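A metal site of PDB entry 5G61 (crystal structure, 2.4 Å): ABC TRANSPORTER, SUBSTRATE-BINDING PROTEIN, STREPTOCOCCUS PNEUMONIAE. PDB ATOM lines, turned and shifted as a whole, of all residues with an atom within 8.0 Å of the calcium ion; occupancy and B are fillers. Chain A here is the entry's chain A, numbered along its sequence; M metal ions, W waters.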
ATOM      1  N   ILE A 203     -28.356 -16.564  -3.013  1.00  0.00           N
ATOM      2  CA  ILE A 203     -28.154 -16.267  -4.435  1.00  0.00           C
ATOM      3  C   ILE A 203     -26.708 -15.807  -4.684  1.00  0.00           C
ATOM      4  O   ILE A 203     -25.946 -16.492  -5.377  1.00  0.00           O
ATOM      5  CB  ILE A 203     -29.209 -15.251  -4.948  1.00  0.00           C
ATOM      6  CG1 ILE A 203     -30.617 -15.771  -4.663  1.00  0.00           C
ATOM      7  CG2 ILE A 203     -29.065 -15.013  -6.472  1.00  0.00           C
ATOM      8  CD1 ILE A 203     -31.756 -14.774  -4.957  1.00  0.00           C
ATOM      9  N   HIS A 209     -23.152 -10.796 -13.146  1.00  0.00           N
ATOM     10  CA  HIS A 209     -24.350 -10.413 -12.405  1.00  0.00           C
ATOM     11  C   HIS A 209     -25.569 -11.185 -12.908  1.00  0.00           C
ATOM     12  O   HIS A 209     -26.673 -10.649 -12.946  1.00  0.00           O
ATOM     13  CB  HIS A 209     -24.579  -8.904 -12.490  1.00  0.00           C
ATOM     14  CG  HIS A 209     -23.354  -8.118 -12.185  1.00  0.00           C
ATOM     15  ND1 HIS A 209     -22.618  -8.317 -11.029  1.00  0.00           N
ATOM     16  CD2 HIS A 209     -22.717  -7.144 -12.867  1.00  0.00           C
ATOM     17  CE1 HIS A 209     -21.597  -7.480 -11.015  1.00  0.00           C
ATOM     18  NE2 HIS A 209     -21.633  -6.751 -12.115  1.00  0.00           N
ATOM     19  N   LEU A 210     -25.343 -12.443 -13.304  1.00  0.00           N
ATOM     20  CA  LEU A 210     -26.358 -13.296 -13.913  1.00  0.00           C
ATOM     21  C   LEU A 210     -26.240 -14.725 -13.383  1.00  0.00           C
ATOM     22  O   LEU A 210     -25.174 -15.347 -13.496  1.00  0.00           O
ATOM     23  CB  LEU A 210     -26.215 -13.322 -15.437  1.00  0.00           C
ATOM     24  CG  LEU A 210     -27.092 -12.379 -16.255  1.00  0.00           C
ATOM     25  CD1 LEU A 210     -27.023 -12.778 -17.722  1.00  0.00           C
ATOM     26  CD2 LEU A 210     -28.549 -12.387 -15.763  1.00  0.00           C
ATOM     27  N   VAL A 211     -27.339 -15.245 -12.837  1.00  0.00           N
ATOM     28  CA  VAL A 211     -27.474 -16.647 -12.507  1.00  0.00           C
ATOM     29  C   VAL A 211     -28.795 -17.154 -13.078  1.00  0.00           C
ATOM     30  O   VAL A 211     -29.665 -16.375 -13.507  1.00  0.00           O
ATOM     31  CB  VAL A 211     -27.367 -16.911 -10.994  1.00  0.00           C
ATOM     32  CG1 VAL A 211     -26.057 -16.396 -10.449  1.00  0.00           C
ATOM     33  CG2 VAL A 211     -28.563 -16.310 -10.231  1.00  0.00           C
ATOM     34  N   VAL A 218     -33.748 -16.609 -15.598  1.00  0.00           N
ATOM     35  CA  VAL A 218     -32.458 -15.976 -15.315  1.00  0.00           C
ATOM     36  C   VAL A 218     -32.673 -14.824 -14.339  1.00  0.00           C
ATOM     37  O   VAL A 218     -33.680 -14.100 -14.414  1.00  0.00           O
ATOM     38  CB  VAL A 218     -31.743 -15.508 -16.583  1.00  0.00           C
ATOM     39  CG1 VAL A 218     -31.850 -16.561 -17.677  1.00  0.00           C
ATOM     40  CG2 VAL A 218     -32.237 -14.145 -17.062  1.00  0.00           C
ATOM     41  N   ASP A 219     -31.736 -14.657 -13.406  1.00  0.00           N
ATOM     42  CA  ASP A 219     -31.820 -13.598 -12.420  1.00  0.00           C
ATOM     43  C   ASP A 219     -30.636 -12.643 -12.578  1.00  0.00           C
ATOM     44  O   ASP A 219     -29.492 -13.052 -12.469  1.00  0.00           O
ATOM     45  CB  ASP A 219     -31.825 -14.138 -10.988  1.00  0.00           C
ATOM     46  CG  ASP A 219     -32.038 -13.017  -9.999  1.00  0.00           C
ATOM     47  OD1 ASP A 219     -32.405 -11.914 -10.442  1.00  0.00           O
ATOM     48  OD2 ASP A 219     -31.883 -13.188  -8.794  1.00  0.00           O
ATOM     49  N   PHE A 220     -30.949 -11.370 -12.767  1.00  0.00           N
ATOM     50  CA  PHE A 220     -29.922 -10.333 -12.616  1.00  0.00           C
ATOM     51  C   PHE A 220     -29.610 -10.188 -11.128  1.00  0.00           C
ATOM     52  O   PHE A 220     -30.433  -9.706 -10.350  1.00  0.00           O
ATOM     53  CB  PHE A 220     -30.385  -9.035 -13.258  1.00  0.00           C
ATOM     54  CG  PHE A 220     -29.403  -7.904 -13.120  1.00  0.00           C
ATOM     55  CD1 PHE A 220     -28.309  -7.801 -13.972  1.00  0.00           C
ATOM     56  CD2 PHE A 220     -29.601  -6.906 -12.169  1.00  0.00           C
ATOM     57  CE1 PHE A 220     -27.425  -6.752 -13.859  1.00  0.00           C
ATOM     58  CE2 PHE A 220     -28.726  -5.841 -12.048  1.00  0.00           C
ATOM     59  CZ  PHE A 220     -27.632  -5.770 -12.886  1.00  0.00           C
ATOM     60  N   THR A 221     -28.418 -10.618 -10.721  1.00  0.00           N
ATOM     61  CA  THR A 221     -28.148 -10.754  -9.299  1.00  0.00           C
ATOM     62  C   THR A 221     -28.053  -9.409  -8.603  1.00  0.00           C
ATOM     63  O   THR A 221     -28.403  -9.308  -7.419  1.00  0.00           O
ATOM     64  CB  THR A 221     -26.854 -11.541  -9.093  1.00  0.00           C
ATOM     65  OG1 THR A 221     -25.777 -10.903  -9.800  1.00  0.00           O
ATOM     66  CG2 THR A 221     -27.012 -12.933  -9.618  1.00  0.00           C
ATOM     67  N   ALA A 222     -27.599  -8.357  -9.301  1.00  0.00           N
ATOM     68  CA  ALA A 222     -27.234  -7.116  -8.611  1.00  0.00           C
ATOM     69  C   ALA A 222     -28.425  -6.208  -8.283  1.00  0.00           C
ATOM     70  O   ALA A 222     -28.204  -5.083  -7.807  1.00  0.00           O
ATOM     71  CB  ALA A 222     -26.170  -6.350  -9.413  1.00  0.00           C
ATOM     72  N   ASP A 223     -29.665  -6.637  -8.489  1.00  0.00           N
ATOM     73  CA  ASP A 223     -30.817  -5.915  -7.970  1.00  0.00           C
ATOM     74  C   ASP A 223     -31.560  -6.688  -6.880  1.00  0.00           C
ATOM     75  O   ASP A 223     -32.620  -6.240  -6.413  1.00  0.00           O
ATOM     76  CB  ASP A 223     -31.743  -5.477  -9.119  1.00  0.00           C
ATOM     77  CG  ASP A 223     -32.513  -6.631  -9.797  1.00  0.00           C
ATOM     78  OD1 ASP A 223     -32.183  -7.826  -9.618  1.00  0.00           O
ATOM     79  OD2 ASP A 223     -33.471  -6.313 -10.541  1.00  0.00           O
ATOM     80  N   ASN A 224     -31.006  -7.800  -6.405  1.00  0.00           N
ATOM     81  CA  ASN A 224     -31.694  -8.564  -5.369  1.00  0.00           C
ATOM     82  C   ASN A 224     -31.510  -7.935  -3.993  1.00  0.00           C
ATOM     83  O   ASN A 224     -30.534  -7.244  -3.709  1.00  0.00           O
ATOM     84  CB  ASN A 224     -31.160 -10.000  -5.303  1.00  0.00           C
ATOM     85  CG  ASN A 224     -31.327 -10.734  -6.602  1.00  0.00           C
ATOM     86  OD1 ASN A 224     -32.184 -10.392  -7.427  1.00  0.00           O
ATOM     87  ND2 ASN A 224     -30.502 -11.752  -6.806  1.00  0.00           N
ATOM     88  N   ASP A 225     -32.466  -8.240  -3.106  1.00  0.00           N
ATOM     89  CA  ASP A 225     -32.318  -7.870  -1.703  1.00  0.00           C
ATOM     90  C   ASP A 225     -31.127  -8.578  -1.067  1.00  0.00           C
ATOM     91  O   ASP A 225     -30.482  -8.022  -0.168  1.00  0.00           O
ATOM     92  CB  ASP A 225     -33.604  -8.186  -0.927  1.00  0.00           C
ATOM     93  CG  ASP A 225     -34.745  -7.276  -1.276  1.00  0.00           C
ATOM     94  OD1 ASP A 225     -34.461  -6.144  -1.726  1.00  0.00           O
ATOM     95  OD2 ASP A 225     -35.913  -7.657  -1.089  1.00  0.00           O
ATOM     96  N   ASN A 226     -30.888  -9.823  -1.475  1.00  0.00           N
ATOM     97  CA  ASN A 226     -29.709 -10.563  -1.042  1.00  0.00           C
ATOM     98  C   ASN A 226     -28.449  -9.808  -1.417  1.00  0.00           C
ATOM     99  O   ASN A 226     -27.465  -9.788  -0.664  1.00  0.00           O
ATOM    100  CB  ASN A 226     -29.682 -11.940  -1.685  1.00  0.00           C
ATOM    101  CG  ASN A 226     -30.996 -12.697  -1.545  1.00  0.00           C
ATOM    102  OD1 ASN A 226     -31.976 -12.366  -2.188  1.00  0.00           O
ATOM    103  ND2 ASN A 226     -31.017 -13.718  -0.708  1.00  0.00           N
ATOM    104  N   TYR A 227     -28.460  -9.198  -2.603  1.00  0.00           N
ATOM    105  CA  TYR A 227     -27.324  -8.425  -3.032  1.00  0.00           C
ATOM    106  C   TYR A 227     -27.132  -7.192  -2.150  1.00  0.00           C
ATOM    107  O   TYR A 227     -26.019  -6.887  -1.744  1.00  0.00           O
ATOM    108  CB  TYR A 227     -27.504  -8.024  -4.502  1.00  0.00           C
ATOM    109  CG  TYR A 227     -26.363  -7.233  -5.063  1.00  0.00           C
ATOM    110  CD1 TYR A 227     -26.320  -5.848  -4.936  1.00  0.00           C
ATOM    111  CD2 TYR A 227     -25.318  -7.869  -5.727  1.00  0.00           C
ATOM    112  CE1 TYR A 227     -25.275  -5.124  -5.474  1.00  0.00           C
ATOM    113  CE2 TYR A 227     -24.289  -7.172  -6.255  1.00  0.00           C
ATOM    114  CZ  TYR A 227     -24.254  -5.793  -6.126  1.00  0.00           C
ATOM    115  OH  TYR A 227     -23.179  -5.097  -6.673  1.00  0.00           O
ATOM    116  N   LYS A 467     -32.287   0.999  -8.420  1.00  0.00           N
ATOM    117  CA  LYS A 467     -33.025   0.051  -9.247  1.00  0.00           C
ATOM    118  C   LYS A 467     -33.775   0.758 -10.379  1.00  0.00           C
ATOM    119  O   LYS A 467     -33.845   0.247 -11.505  1.00  0.00           O
ATOM    120  CB  LYS A 467     -33.967  -0.779  -8.378  1.00  0.00           C
ATOM    121  CG  LYS A 467     -33.264  -1.599  -7.301  1.00  0.00           C
ATOM    122  CD  LYS A 467     -34.142  -2.767  -6.791  1.00  0.00           C
ATOM    123  CE  LYS A 467     -35.206  -2.315  -5.754  1.00  0.00           C
ATOM    124  NZ  LYS A 467     -36.101  -3.430  -5.267  1.00  0.00           N
ATOM    125  N   LEU A 475     -32.587  -2.607 -17.982  1.00  0.00           N
ATOM    126  CA  LEU A 475     -32.416  -3.929 -17.380  1.00  0.00           C
ATOM    127  C   LEU A 475     -33.477  -4.896 -17.888  1.00  0.00           C
ATOM    128  O   LEU A 475     -33.152  -6.004 -18.319  1.00  0.00           O
ATOM    129  CB  LEU A 475     -32.448  -3.813 -15.856  1.00  0.00           C
ATOM    130  CG  LEU A 475     -32.192  -5.108 -15.082  1.00  0.00           C
ATOM    131  CD1 LEU A 475     -30.885  -5.725 -15.528  1.00  0.00           C
ATOM    132  CD2 LEU A 475     -32.213  -4.837 -13.579  1.00  0.00           C
ATOM    133  N   LEU A 479     -32.597  -8.161 -19.560  1.00  0.00           N
ATOM    134  CA  LEU A 479     -32.958  -9.445 -18.995  1.00  0.00           C
ATOM    135  C   LEU A 479     -33.840 -10.228 -19.942  1.00  0.00           C
ATOM    136  O   LEU A 479     -33.755 -11.467 -19.984  1.00  0.00           O
ATOM    137  CB  LEU A 479     -33.640  -9.204 -17.647  1.00  0.00           C
ATOM    138  CG  LEU A 479     -33.333 -10.091 -16.444  1.00  0.00           C
ATOM    139  CD1 LEU A 479     -31.877 -10.478 -16.370  1.00  0.00           C
ATOM    140  CD2 LEU A 479     -33.726  -9.329 -15.172  1.00  0.00           C
HETATM  141 CA    CA M   1     -32.876 -10.064  -9.649  1.00  0.00          CA
HETATM  142  O   HOH W   1     -33.510 -10.041 -11.950  1.00  0.00           O
HETATM  143  O   HOH W   2     -34.872 -11.671  -9.231  1.00  0.00           O
HETATM  144  O   HOH W   3     -35.010  -9.104  -9.060  1.00  0.00           O
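The backbone NH (N) of Asp 219 sits at hydrogen-bond distance from the backbone carbonyl oxygen (O) of Val 211 (2.7 Å). The side-chain amide nitrogen (ND2) of Asn 224 is in hydrogen-bond range of the backbone carbonyl oxygen (O) of Thr 221 (3.3 Å).
The calcium ion is bound by OD1 of Asp 219 (2.1 Å), OD1 of Asp 223 (2.3 Å), OD1 of Asn 224 (2.4 Å), water W1 (2.4 Å), water W3 (2.4 Å), O of Phe 220 (2.6 Å) and water W2 (2.6 Å).
The nearest printed residue that does not touch the calcium ion is Thr 221 (4.6 Å).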
